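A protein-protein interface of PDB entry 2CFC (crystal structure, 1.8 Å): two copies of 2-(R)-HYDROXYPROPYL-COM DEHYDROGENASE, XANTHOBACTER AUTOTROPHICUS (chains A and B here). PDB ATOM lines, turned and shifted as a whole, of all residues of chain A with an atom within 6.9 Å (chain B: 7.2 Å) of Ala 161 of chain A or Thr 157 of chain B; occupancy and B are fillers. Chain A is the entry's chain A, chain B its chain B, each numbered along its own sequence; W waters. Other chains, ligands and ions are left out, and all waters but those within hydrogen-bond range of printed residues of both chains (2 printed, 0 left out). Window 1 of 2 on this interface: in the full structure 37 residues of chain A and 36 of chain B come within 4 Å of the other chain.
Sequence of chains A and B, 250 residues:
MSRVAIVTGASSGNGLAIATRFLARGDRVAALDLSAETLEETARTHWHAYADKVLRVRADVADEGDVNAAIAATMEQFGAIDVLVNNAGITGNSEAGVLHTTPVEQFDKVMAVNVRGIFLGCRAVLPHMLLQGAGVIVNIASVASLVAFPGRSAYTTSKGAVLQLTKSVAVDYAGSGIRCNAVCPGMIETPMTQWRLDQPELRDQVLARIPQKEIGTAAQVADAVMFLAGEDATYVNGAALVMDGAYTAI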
ATOM      1  N   MET A 111      25.730 -20.309  -1.612  1.00  0.00           N
ATOM      2  CA  MET A 111      24.980 -21.566  -1.547  1.00  0.00           C
ATOM      3  C   MET A 111      25.579 -22.563  -0.549  1.00  0.00           C
ATOM      4  O   MET A 111      24.830 -23.303   0.127  1.00  0.00           O
ATOM      5  CB  MET A 111      24.907 -22.211  -2.931  1.00  0.00           C
ATOM      6  CG  MET A 111      24.094 -21.361  -3.947  1.00  0.00           C
ATOM      7  SD  MET A 111      22.380 -21.148  -3.529  1.00  0.00           S
ATOM      8  CE  MET A 111      21.730 -22.829  -3.905  1.00  0.00           C
ATOM      9  N   ASN A 114      24.785 -20.871   3.169  1.00  0.00           N
ATOM     10  CA  ASN A 114      23.358 -20.727   3.432  1.00  0.00           C
ATOM     11  C   ASN A 114      22.528 -21.971   3.245  1.00  0.00           C
ATOM     12  O   ASN A 114      21.500 -22.127   3.910  1.00  0.00           O
ATOM     13  CB  ASN A 114      22.784 -19.608   2.560  1.00  0.00           C
ATOM     14  CG  ASN A 114      23.303 -18.238   2.939  1.00  0.00           C
ATOM     15  OD1 ASN A 114      24.223 -18.111   3.747  1.00  0.00           O
ATOM     16  ND2 ASN A 114      22.712 -17.192   2.352  1.00  0.00           N
ATOM     17  N   VAL A 115      22.953 -22.865   2.347  1.00  0.00           N
ATOM     18  CA  VAL A 115      22.167 -24.075   2.090  1.00  0.00           C
ATOM     19  C   VAL A 115      22.898 -25.357   2.498  1.00  0.00           C
ATOM     20  O   VAL A 115      22.383 -26.162   3.295  1.00  0.00           O
ATOM     21  CB  VAL A 115      21.778 -24.188   0.598  1.00  0.00           C
ATOM     22  CG1 VAL A 115      20.821 -25.346   0.398  1.00  0.00           C
ATOM     23  CG2 VAL A 115      21.164 -22.863   0.063  1.00  0.00           C
ATOM     24  N   PHE A 119      21.935 -28.134   5.389  1.00  0.00           N
ATOM     25  CA  PHE A 119      21.797 -29.567   5.091  1.00  0.00           C
ATOM     26  C   PHE A 119      22.755 -30.376   5.997  1.00  0.00           C
ATOM     27  O   PHE A 119      22.360 -31.379   6.603  1.00  0.00           O
ATOM     28  CB  PHE A 119      22.142 -29.848   3.611  1.00  0.00           C
ATOM     29  CG  PHE A 119      22.398 -31.305   3.304  1.00  0.00           C
ATOM     30  CD1 PHE A 119      21.340 -32.212   3.189  1.00  0.00           C
ATOM     31  CD2 PHE A 119      23.704 -31.769   3.136  1.00  0.00           C
ATOM     32  CE1 PHE A 119      21.601 -33.589   2.903  1.00  0.00           C
ATOM     33  CE2 PHE A 119      23.970 -33.134   2.856  1.00  0.00           C
ATOM     34  CZ  PHE A 119      22.911 -34.033   2.741  1.00  0.00           C
ATOM     35  N   SER A 145      12.922 -15.828   0.860  1.00  0.00           N
ATOM     36  CA  SER A 145      12.548 -17.210   0.530  1.00  0.00           C
ATOM     37  C   SER A 145      11.221 -17.130  -0.204  1.00  0.00           C
ATOM     38  O   SER A 145      10.820 -18.091  -0.874  1.00  0.00           O
ATOM     39  CB  SER A 145      12.307 -18.070   1.785  1.00  0.00           C
ATOM     40  OG  SER A 145      13.481 -18.269   2.564  1.00  0.00           O
ATOM     41  N   THR A 156      18.995 -14.592  -2.503  1.00  0.00           N
ATOM     42  CA  THR A 156      17.580 -14.898  -2.716  1.00  0.00           C
ATOM     43  C   THR A 156      17.440 -16.374  -3.098  1.00  0.00           C
ATOM     44  O   THR A 156      16.609 -17.108  -2.537  1.00  0.00           O
ATOM     45  CB  THR A 156      16.999 -13.973  -3.816  1.00  0.00           C
ATOM     46  OG1 THR A 156      16.971 -12.625  -3.309  1.00  0.00           O
ATOM     47  CG2 THR A 156      15.544 -14.405  -4.215  1.00  0.00           C
ATOM     48  N   THR A 157      18.288 -16.817  -4.019  1.00  0.00           N
ATOM     49  CA  THR A 157      18.268 -18.207  -4.464  1.00  0.00           C
ATOM     50  C   THR A 157      18.473 -19.161  -3.294  1.00  0.00           C
ATOM     51  O   THR A 157      17.700 -20.137  -3.129  1.00  0.00           O
ATOM     52  CB  THR A 157      19.377 -18.449  -5.470  1.00  0.00           C
ATOM     53  OG1 THR A 157      19.148 -17.620  -6.615  1.00  0.00           O
ATOM     54  CG2 THR A 157      19.396 -19.883  -5.919  1.00  0.00           C
ATOM     55  N   SER A 158      19.484 -18.866  -2.476  1.00  0.00           N
ATOM     56  CA  SER A 158      19.810 -19.726  -1.336  1.00  0.00           C
ATOM     57  C   SER A 158      18.647 -19.835  -0.356  1.00  0.00           C
ATOM     58  O   SER A 158      18.374 -20.923   0.168  1.00  0.00           O
ATOM     59  CB  SER A 158      21.071 -19.215  -0.610  1.00  0.00           C
ATOM     60  OG  SER A 158      20.832 -18.040   0.175  1.00  0.00           O
ATOM     61  N   LYS A 159      17.936 -18.732  -0.125  1.00  0.00           N
ATOM     62  CA  LYS A 159      16.844 -18.746   0.840  1.00  0.00           C
ATOM     63  C   LYS A 159      15.620 -19.503   0.350  1.00  0.00           C
ATOM     64  O   LYS A 159      14.851 -20.020   1.162  1.00  0.00           O
ATOM     65  CB  LYS A 159      16.507 -17.313   1.287  1.00  0.00           C
ATOM     66  CG  LYS A 159      17.657 -16.677   2.115  1.00  0.00           C
ATOM     67  CD  LYS A 159      17.922 -17.406   3.438  1.00  0.00           C
ATOM     68  CE  LYS A 159      19.067 -16.728   4.185  1.00  0.00           C
ATOM     69  NZ  LYS A 159      19.343 -17.407   5.488  1.00  0.00           N
ATOM     70  N   GLY A 160      15.429 -19.577  -0.968  1.00  0.00           N
ATOM     71  CA  GLY A 160      14.347 -20.396  -1.480  1.00  0.00           C
ATOM     72  C   GLY A 160      14.645 -21.861  -1.131  1.00  0.00           C
ATOM     73  O   GLY A 160      13.746 -22.631  -0.794  1.00  0.00           O
ATOM     74  N   ALA A 161      15.907 -22.267  -1.222  1.00  0.00           N
ATOM     75  CA  ALA A 161      16.276 -23.630  -0.869  1.00  0.00           C
ATOM     76  C   ALA A 161      16.120 -23.848   0.646  1.00  0.00           C
ATOM     77  O   ALA A 161      15.696 -24.919   1.080  1.00  0.00           O
ATOM     78  CB  ALA A 161      17.740 -23.926  -1.315  1.00  0.00           C
ATOM     79  N   VAL A 162      16.430 -22.838   1.457  1.00  0.00           N
ATOM     80  CA  VAL A 162      16.299 -23.016   2.910  1.00  0.00           C
ATOM     81  C   VAL A 162      14.843 -23.312   3.291  1.00  0.00           C
ATOM     82  O   VAL A 162      14.567 -24.225   4.082  1.00  0.00           O
ATOM     83  CB  VAL A 162      16.771 -21.764   3.693  1.00  0.00           C
ATOM     84  CG1 VAL A 162      16.591 -21.996   5.238  1.00  0.00           C
ATOM     85  CG2 VAL A 162      18.254 -21.503   3.394  1.00  0.00           C
ATOM     86  N   LEU A 163      13.899 -22.569   2.714  1.00  0.00           N
ATOM     87  CA  LEU A 163      12.501 -22.797   3.037  1.00  0.00           C
ATOM     88  C   LEU A 163      12.028 -24.196   2.638  1.00  0.00           C
ATOM     89  O   LEU A 163      11.303 -24.851   3.402  1.00  0.00           O
ATOM     90  CB  LEU A 163      11.628 -21.731   2.351  1.00  0.00           C
ATOM     91  CG  LEU A 163      10.098 -21.835   2.557  1.00  0.00           C
ATOM     92  CD1 LEU A 163       9.756 -21.810   4.025  1.00  0.00           C
ATOM     93  CD2 LEU A 163       9.412 -20.682   1.800  1.00  0.00           C
ATOM     94  N   GLN A 164      12.420 -24.662   1.448  1.00  0.00           N
ATOM     95  CA  GLN A 164      11.980 -25.989   1.017  1.00  0.00           C
ATOM     96  C   GLN A 164      12.646 -27.121   1.780  1.00  0.00           C
ATOM     97  O   GLN A 164      12.032 -28.172   1.992  1.00  0.00           O
ATOM     98  CB  GLN A 164      12.163 -26.154  -0.503  1.00  0.00           C
ATOM     99  CG  GLN A 164      11.078 -25.380  -1.283  1.00  0.00           C
ATOM    100  CD  GLN A 164       9.678 -25.666  -0.780  1.00  0.00           C
ATOM    101  OE1 GLN A 164       9.070 -26.702  -1.110  1.00  0.00           O
ATOM    102  NE2 GLN A 164       9.145 -24.747   0.010  1.00  0.00           N
ATOM    103  N   LEU A 165      13.908 -26.928   2.170  1.00  0.00           N
ATOM    104  CA  LEU A 165      14.605 -27.929   2.962  1.00  0.00           C
ATOM    105  C   LEU A 165      13.834 -28.017   4.281  1.00  0.00           C
ATOM    106  O   LEU A 165      13.630 -29.109   4.829  1.00  0.00           O
ATOM    107  CB  LEU A 165      16.053 -27.489   3.211  1.00  0.00           C
ATOM    108  CG  LEU A 165      16.908 -28.416   4.055  1.00  0.00           C
ATOM    109  CD1 LEU A 165      18.409 -28.151   3.745  1.00  0.00           C
ATOM    110  CD2 LEU A 165      16.617 -28.157   5.554  1.00  0.00           C
ATOM    111  N   THR A 166      13.408 -26.868   4.805  1.00  0.00           N
ATOM    112  CA  THR A 166      12.645 -26.860   6.045  1.00  0.00           C
ATOM    113  C   THR A 166      11.393 -27.743   5.939  1.00  0.00           C
ATOM    114  O   THR A 166      11.137 -28.605   6.824  1.00  0.00           O
ATOM    115  CB  THR A 166      12.211 -25.437   6.390  1.00  0.00           C
ATOM    116  OG1 THR A 166      13.382 -24.618   6.547  1.00  0.00           O
ATOM    117  CG2 THR A 166      11.412 -25.426   7.662  1.00  0.00           C
ATOM    118  N   LYS A 167      10.624 -27.537   4.869  1.00  0.00           N
ATOM    119  CA  LYS A 167       9.409 -28.311   4.637  1.00  0.00           C
ATOM    120  C   LYS A 167       9.725 -29.779   4.433  1.00  0.00           C
ATOM    121  O   LYS A 167       8.951 -30.633   4.868  1.00  0.00           O
ATOM    122  CB  LYS A 167       8.627 -27.772   3.429  1.00  0.00           C
ATOM    123  CG  LYS A 167       8.136 -26.346   3.652  1.00  0.00           C
ATOM    124  CD  LYS A 167       7.177 -25.880   2.585  1.00  0.00           C
ATOM    125  CE  LYS A 167       6.936 -24.398   2.743  1.00  0.00           C
ATOM    126  NZ  LYS A 167       6.196 -23.867   1.576  1.00  0.00           N
ATOM    127  N   SER A 168      10.860 -30.076   3.796  1.00  0.00           N
ATOM    128  CA  SER A 168      11.261 -31.462   3.559  1.00  0.00           C
ATOM    129  C   SER A 168      11.486 -32.209   4.882  1.00  0.00           C
ATOM    130  O   SER A 168      10.962 -33.315   5.092  1.00  0.00           O
ATOM    131  CB  SER A 168      12.532 -31.501   2.717  1.00  0.00           C
ATOM    132  OG  SER A 168      13.091 -32.803   2.713  1.00  0.00           O
ATOM    133  N   LEU B  99      16.444 -36.472   4.233  1.00  0.00           N
ATOM    134  CA  LEU B  99      17.690 -35.747   4.438  1.00  0.00           C
ATOM    135  C   LEU B  99      18.853 -36.439   5.136  1.00  0.00           C
ATOM    136  O   LEU B  99      19.950 -36.507   4.565  1.00  0.00           O
ATOM    137  CB  LEU B  99      17.410 -34.410   5.141  1.00  0.00           C
ATOM    138  CG  LEU B  99      18.551 -33.370   5.127  1.00  0.00           C
ATOM    139  CD1 LEU B  99      17.903 -32.001   5.376  1.00  0.00           C
ATOM    140  CD2 LEU B  99      19.641 -33.654   6.175  1.00  0.00           C
ATOM    141  N   PHE B 107      23.631 -34.850  -2.449  1.00  0.00           N
ATOM    142  CA  PHE B 107      23.064 -33.543  -2.211  1.00  0.00           C
ATOM    143  C   PHE B 107      23.831 -32.537  -3.092  1.00  0.00           C
ATOM    144  O   PHE B 107      23.219 -31.734  -3.790  1.00  0.00           O
ATOM    145  CB  PHE B 107      23.213 -33.153  -0.741  1.00  0.00           C
ATOM    146  CG  PHE B 107      22.811 -31.735  -0.455  1.00  0.00           C
ATOM    147  CD1 PHE B 107      21.487 -31.420  -0.174  1.00  0.00           C
ATOM    148  CD2 PHE B 107      23.752 -30.710  -0.507  1.00  0.00           C
ATOM    149  CE1 PHE B 107      21.095 -30.088   0.055  1.00  0.00           C
ATOM    150  CE2 PHE B 107      23.384 -29.379  -0.283  1.00  0.00           C
ATOM    151  CZ  PHE B 107      22.056 -29.070  -0.003  1.00  0.00           C
ATOM    152  N   VAL B 110      22.865 -32.935  -6.886  1.00  0.00           N
ATOM    153  CA  VAL B 110      21.527 -32.445  -7.204  1.00  0.00           C
ATOM    154  C   VAL B 110      21.506 -30.918  -7.191  1.00  0.00           C
ATOM    155  O   VAL B 110      20.930 -30.304  -8.113  1.00  0.00           O
ATOM    156  CB  VAL B 110      20.469 -33.045  -6.226  1.00  0.00           C
ATOM    157  CG1 VAL B 110      19.076 -32.349  -6.383  1.00  0.00           C
ATOM    158  CG2 VAL B 110      20.382 -34.528  -6.475  1.00  0.00           C
ATOM    159  N   MET B 111      22.120 -30.299  -6.177  1.00  0.00           N
ATOM    160  CA  MET B 111      22.188 -28.828  -6.123  1.00  0.00           C
ATOM    161  C   MET B 111      23.020 -28.247  -7.288  1.00  0.00           C
ATOM    162  O   MET B 111      22.686 -27.185  -7.824  1.00  0.00           O
ATOM    163  CB  MET B 111      22.804 -28.357  -4.792  1.00  0.00           C
ATOM    164  CG  MET B 111      21.934 -28.708  -3.554  1.00  0.00           C
ATOM    165  SD  MET B 111      20.336 -27.970  -3.600  1.00  0.00           S
ATOM    166  CE  MET B 111      20.778 -26.283  -3.358  1.00  0.00           C
ATOM    167  N   VAL B 115      20.428 -26.325  -9.606  1.00  0.00           N
ATOM    168  CA  VAL B 115      20.494 -24.905  -9.257  1.00  0.00           C
ATOM    169  C   VAL B 115      21.699 -24.221  -9.894  1.00  0.00           C
ATOM    170  O   VAL B 115      21.538 -23.248 -10.656  1.00  0.00           O
ATOM    171  CB  VAL B 115      20.565 -24.701  -7.731  1.00  0.00           C
ATOM    172  CG1 VAL B 115      20.391 -23.254  -7.401  1.00  0.00           C
ATOM    173  CG2 VAL B 115      19.526 -25.587  -7.005  1.00  0.00           C
ATOM    174  N   ALA B 144       7.501 -29.200  -6.080  1.00  0.00           N
ATOM    175  CA  ALA B 144       8.395 -29.355  -4.929  1.00  0.00           C
ATOM    176  C   ALA B 144       9.047 -28.008  -4.541  1.00  0.00           C
ATOM    177  O   ALA B 144       9.726 -27.909  -3.524  1.00  0.00           O
ATOM    178  CB  ALA B 144       9.469 -30.404  -5.204  1.00  0.00           C
ATOM    179  N   SER B 145       8.824 -26.989  -5.366  1.00  0.00           N
ATOM    180  CA  SER B 145       9.310 -25.638  -5.098  1.00  0.00           C
ATOM    181  C   SER B 145       8.351 -25.035  -4.078  1.00  0.00           C
ATOM    182  O   SER B 145       8.711 -24.074  -3.391  1.00  0.00           O
ATOM    183  CB  SER B 145       9.228 -24.765  -6.356  1.00  0.00           C
ATOM    184  OG  SER B 145      10.128 -25.167  -7.365  1.00  0.00           O
ATOM    185  N   ARG B 152      12.334 -37.099  -0.811  1.00  0.00           N
ATOM    186  CA  ARG B 152      13.171 -36.550  -1.866  1.00  0.00           C
ATOM    187  C   ARG B 152      13.617 -35.187  -1.369  1.00  0.00           C
ATOM    188  O   ARG B 152      13.238 -34.164  -1.924  1.00  0.00           O
ATOM    189  CB  ARG B 152      12.357 -36.429  -3.168  1.00  0.00           C
ATOM    190  CG  ARG B 152      12.153 -37.773  -3.897  1.00  0.00           C
ATOM    191  CD  ARG B 152      13.512 -38.384  -4.319  1.00  0.00           C
ATOM    192  NE  ARG B 152      13.388 -39.411  -5.358  1.00  0.00           N
ATOM    193  CZ  ARG B 152      14.397 -40.148  -5.828  1.00  0.00           C
ATOM    194  NH1 ARG B 152      15.632 -39.993  -5.357  1.00  0.00           N
ATOM    195  NH2 ARG B 152      14.171 -41.037  -6.793  1.00  0.00           N
ATOM    196  N   SER B 153      14.466 -35.182  -0.347  1.00  0.00           N
ATOM    197  CA  SER B 153      14.893 -33.934   0.286  1.00  0.00           C
ATOM    198  C   SER B 153      15.813 -33.023  -0.544  1.00  0.00           C
ATOM    199  O   SER B 153      15.575 -31.809  -0.655  1.00  0.00           O
ATOM    200  CB  SER B 153      15.546 -34.272   1.642  1.00  0.00           C
ATOM    201  OG  SER B 153      15.974 -33.098   2.322  1.00  0.00           O
ATOM    202  N   ALA B 154      16.863 -33.587  -1.122  1.00  0.00           N
ATOM    203  CA  ALA B 154      17.774 -32.786  -1.934  1.00  0.00           C
ATOM    204  C   ALA B 154      17.033 -32.196  -3.113  1.00  0.00           C
ATOM    205  O   ALA B 154      17.223 -31.039  -3.447  1.00  0.00           O
ATOM    206  CB  ALA B 154      18.895 -33.621  -2.435  1.00  0.00           C
ATOM    207  N   TYR B 155      16.213 -33.005  -3.776  1.00  0.00           N
ATOM    208  CA  TYR B 155      15.453 -32.524  -4.923  1.00  0.00           C
ATOM    209  C   TYR B 155      14.521 -31.383  -4.493  1.00  0.00           C
ATOM    210  O   TYR B 155      14.434 -30.342  -5.157  1.00  0.00           O
ATOM    211  CB  TYR B 155      14.610 -33.659  -5.497  1.00  0.00           C
ATOM    212  CG  TYR B 155      13.741 -33.222  -6.655  1.00  0.00           C
ATOM    213  CD1 TYR B 155      14.232 -33.242  -7.958  1.00  0.00           C
ATOM    214  CD2 TYR B 155      12.416 -32.831  -6.447  1.00  0.00           C
ATOM    215  CE1 TYR B 155      13.419 -32.896  -9.030  1.00  0.00           C
ATOM    216  CE2 TYR B 155      11.595 -32.477  -7.513  1.00  0.00           C
ATOM    217  CZ  TYR B 155      12.097 -32.516  -8.797  1.00  0.00           C
ATOM    218  OH  TYR B 155      11.282 -32.182  -9.847  1.00  0.00           O
ATOM    219  N   THR B 156      13.799 -31.587  -3.398  1.00  0.00           N
ATOM    220  CA  THR B 156      12.880 -30.563  -2.911  1.00  0.00           C
ATOM    221  C   THR B 156      13.634 -29.263  -2.590  1.00  0.00           C
ATOM    222  O   THR B 156      13.192 -28.165  -2.949  1.00  0.00           O
ATOM    223  CB  THR B 156      12.132 -31.062  -1.647  1.00  0.00           C
ATOM    224  OG1 THR B 156      11.208 -32.093  -2.046  1.00  0.00           O
ATOM    225  CG2 THR B 156      11.332 -29.902  -0.973  1.00  0.00           C
ATOM    226  N   THR B 157      14.789 -29.404  -1.963  1.00  0.00           N
ATOM    227  CA  THR B 157      15.630 -28.255  -1.610  1.00  0.00           C
ATOM    228  C   THR B 157      16.057 -27.466  -2.855  1.00  0.00           C
ATOM    229  O   THR B 157      15.919 -26.234  -2.902  1.00  0.00           O
ATOM    230  CB  THR B 157      16.878 -28.743  -0.856  1.00  0.00           C
ATOM    231  OG1 THR B 157      16.462 -29.386   0.363  1.00  0.00           O
ATOM    232  CG2 THR B 157      17.820 -27.586  -0.536  1.00  0.00           C
ATOM    233  N   SER B 158      16.572 -28.183  -3.857  1.00  0.00           N
ATOM    234  CA  SER B 158      17.005 -27.554  -5.120  1.00  0.00           C
ATOM    235  C   SER B 158      15.878 -26.759  -5.797  1.00  0.00           C
ATOM    236  O   SER B 158      16.111 -25.680  -6.318  1.00  0.00           O
ATOM    237  CB  SER B 158      17.524 -28.638  -6.097  1.00  0.00           C
ATOM    238  OG  SER B 158      16.454 -29.438  -6.598  1.00  0.00           O
ATOM    239  N   LYS B 159      14.654 -27.285  -5.797  1.00  0.00           N
ATOM    240  CA  LYS B 159      13.541 -26.621  -6.456  1.00  0.00           C
ATOM    241  C   LYS B 159      13.091 -25.355  -5.735  1.00  0.00           C
ATOM    242  O   LYS B 159      12.569 -24.439  -6.359  1.00  0.00           O
ATOM    243  CB  LYS B 159      12.406 -27.622  -6.672  1.00  0.00           C
ATOM    244  CG  LYS B 159      12.803 -28.775  -7.646  1.00  0.00           C
ATOM    245  CD  LYS B 159      13.107 -28.230  -9.050  1.00  0.00           C
ATOM    246  CE  LYS B 159      13.487 -29.365 -10.028  1.00  0.00           C
ATOM    247  NZ  LYS B 159      13.732 -28.863 -11.441  1.00  0.00           N
ATOM    248  N   GLY B 160      13.316 -25.290  -4.427  1.00  0.00           N
ATOM    249  CA  GLY B 160      13.008 -24.082  -3.685  1.00  0.00           C
ATOM    250  C   GLY B 160      13.944 -22.981  -4.201  1.00  0.00           C
ATOM    251  O   GLY B 160      13.518 -21.836  -4.406  1.00  0.00           O
ATOM    252  N   ALA B 161      15.211 -23.317  -4.438  1.00  0.00           N
ATOM    253  CA  ALA B 161      16.187 -22.349  -4.984  1.00  0.00           C
ATOM    254  C   ALA B 161      15.842 -21.966  -6.438  1.00  0.00           C
ATOM    255  O   ALA B 161      16.010 -20.801  -6.832  1.00  0.00           O
ATOM    256  CB  ALA B 161      17.618 -22.934  -4.938  1.00  0.00           C
ATOM    257  N   VAL B 162      15.382 -22.924  -7.251  1.00  0.00           N
ATOM    258  CA  VAL B 162      15.035 -22.579  -8.631  1.00  0.00           C
ATOM    259  C   VAL B 162      13.918 -21.516  -8.687  1.00  0.00           C
ATOM    260  O   VAL B 162      14.004 -20.539  -9.456  1.00  0.00           O
ATOM    261  CB  VAL B 162      14.559 -23.835  -9.424  1.00  0.00           C
ATOM    262  CG1 VAL B 162      14.021 -23.430 -10.850  1.00  0.00           C
ATOM    263  CG2 VAL B 162      15.718 -24.819  -9.527  1.00  0.00           C
ATOM    264  N   GLN B 164      13.079 -19.266  -6.452  1.00  0.00           N
ATOM    265  CA  GLN B 164      13.562 -17.961  -5.989  1.00  0.00           C
ATOM    266  C   GLN B 164      14.552 -17.314  -6.946  1.00  0.00           C
ATOM    267  O   GLN B 164      14.570 -16.079  -7.112  1.00  0.00           O
ATOM    268  CB  GLN B 164      14.117 -18.065  -4.553  1.00  0.00           C
ATOM    269  CG  GLN B 164      12.972 -18.191  -3.506  1.00  0.00           C
ATOM    270  CD  GLN B 164      11.876 -17.133  -3.707  1.00  0.00           C
ATOM    271  OE1 GLN B 164      12.042 -15.944  -3.370  1.00  0.00           O
ATOM    272  NE2 GLN B 164      10.758 -17.558  -4.272  1.00  0.00           N
HETATM  273  O   HOH W   1      14.111 -34.772   4.605  1.00  0.00           O
HETATM  274  O   HOH W   2      11.724 -34.586   1.365  1.00  0.00           O
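The backbone carbonyl oxygen (O) of Ser 145 of chain A sits close to the side-chain amide nitrogen (NE2) of Gln 164 of chain B (3.4 Å). The side-chain amide oxygen (OE1) of Gln 164 of chain A lies close to the backbone carbonyl oxygen (O) of Ala 144 of chain B (2.8 Å). The side-chain amide nitrogen of Gln 164 of chain A lies close to the backbone carbonyl oxygen of Ser 145 of chain B (3.5 Å). The side-chain hydroxyl of Ser 153 of chain B lies within hydrogen-bond range of the side-chain hydroxyl of Ser 168 of chain A, at 2.9 Å. The backbone NH (N) of Ala 161 of chain A sits close to the backbone NH (N) of Ala 161 of chain B (3.5 Å).
O of Lys 159 of chain A sits at hydrogen-bond distance from OG of Ser 145 of chain A. NE2 of Gln 164 of chain A sits close to NZ of Lys 167 of chain A, at 3.5 Å. N of Ser 158 of chain B sits close to SD of Met 111 of chain B (3.8 Å). The side-chain hydroxyl of Ser 145 of chain B lies within hydrogen-bond range of the backbone carbonyl oxygen of Lys 159 of chain B. The side-chain hydroxyl (OG1) of Thr 156 of chain B is in hydrogen-bond range of the backbone carbonyl oxygen (O) of Arg 152 of chain B, at 2.9 Å. The side-chain hydroxyl (OG1) of Thr 157 of chain B lies within hydrogen-bond range of the backbone carbonyl oxygen (O) of Ser 153 of chain B.
Among the printed residues, pairs that only touch across the chains: Met 111 of chain A with Met 111 of chain B (3.6 Å), Met 111 of chain A with Val 115 of chain B (3.8 Å), Val 115 of chain A with Phe 107 of chain B (3.9 Å), Val 115 of chain A with Met 111 of chain B (3.9 Å), Val 115 of chain A with Thr 157 of chain B (3.9 Å), Phe 119 of chain A with Leu 99 of chain B (3.6 Å), Phe 119 of chain A with Phe 107 of chain B (3.5 Å), Thr 156 of chain A with Gln 164 of chain B (3.3 Å), Thr 157 of chain A with Val 115 of chain B (3.8 Å), Thr 157 of chain A with Ala 161 of chain B (3.3 Å), Gly 160 of chain A with Gly 160 of chain B (3.3 Å), Gly 160 of chain A with Ala 161 of chain B (3.7 Å), Gly 160 of chain A with Gln 164 of chain B (3.3 Å), Ala 161 of chain A with Thr 157 of chain B (3.3 Å), Ala 161 of chain A with Gly 160 of chain B (3.6 Å), Gln 164 of chain A with Thr 156 of chain B (3.3 Å), Gln 164 of chain A with Gly 160 of chain B (3.3 Å), Leu 165 of chain A with Leu 99 of chain B (3.9 Å) and Leu 165 of chain A with Thr 157 of chain B (3.4 Å).
Of chain B, only Thr 157 (3.3 Å), Gly 160 (3.6 Å) and Ala 161 (3.5 Å) come within 4 Å of Ala 161 of chain A. Thr 157 of chain B touches just these residues of chain A: Val 115, Ala 161 and Leu 165. Printed residues of chain B within 4 Å of Gly 160 of chain A: Gly 160 (3.3 Å), Ala 161 (3.7 Å) and Gln 164 (3.3 Å). Of the printed residues of chain A, Gly 160 of chain B touches Gly 160 (3.3 Å), Ala 161 (3.6 Å) and Gln 164 (3.3 Å). Printed residues of chain A within 4 Å of Ser 153 of chain B: Ser 168 (2.9 Å). Of the printed residues of chain A, Ala 161 of chain B touches Thr 157 (3.3 Å), Gly 160 (3.7 Å) and Ala 161 (3.5 Å). The nearest residue of chain B that does not touch Ala 161 of chain A is Met 111 of chain B (4.4 Å). The nearest residue of chain A that does not touch Thr 157 of chain B is Gln 164 of chain A (4.2 Å). The nearest printed residue of chain A that does not touch Phe 107 of chain B is Leu 165 of chain A (5.0 Å).
Hydrophobic or aromatic side chains of chain B within 4 Å of the printed part of chain A: Leu 99, Phe 107, Met 111, Val 115 and Ala 161. Among the printed residues, no Asp or Glu carboxylate lies within 4 Å of a Lys or Arg side-chain nitrogen of the other chain.
Val 115 of chain A touches Thr 157 of chain B, and with the chains exchanged Thr 157 of chain A touches Val 115 of chain B. Thr 156 of chain A touches Gln 164 of chain B, and with the chains exchanged Gln 164 of chain A touches Thr 156 of chain B. Gly 160 of chain A touches Gln 164 of chain B, and with the chains exchanged Gln 164 of chain A touches Gly 160 of chain B. Ala 161 of chain B touches its own counterpart, Ala 161 of chain A. Positions printed for both chains: 111, 115, 145, 156, 157, 158, 159, 160, 161, 162 and 164. Of the 24 pairs that touch across the chains among the printed residues, 17 have their exchanged pair printed and touching as well.
Water W2 lies within hydrogen-bond range of the side-chain hydroxyl of Ser 168 of chain A (2.6 Å), the backbone NH of Ser 153 of chain B (3.3 Å) and the backbone NH of Arg 152 of chain B (3.4 Å). Water W1 lies within hydrogen-bond range of the backbone NH of Leu 99 of chain B (2.9 Å), the side-chain hydroxyl of Ser 168 of chain A (2.9 Å) and the side-chain hydroxyl of Ser 153 of chain B (3.4 Å).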
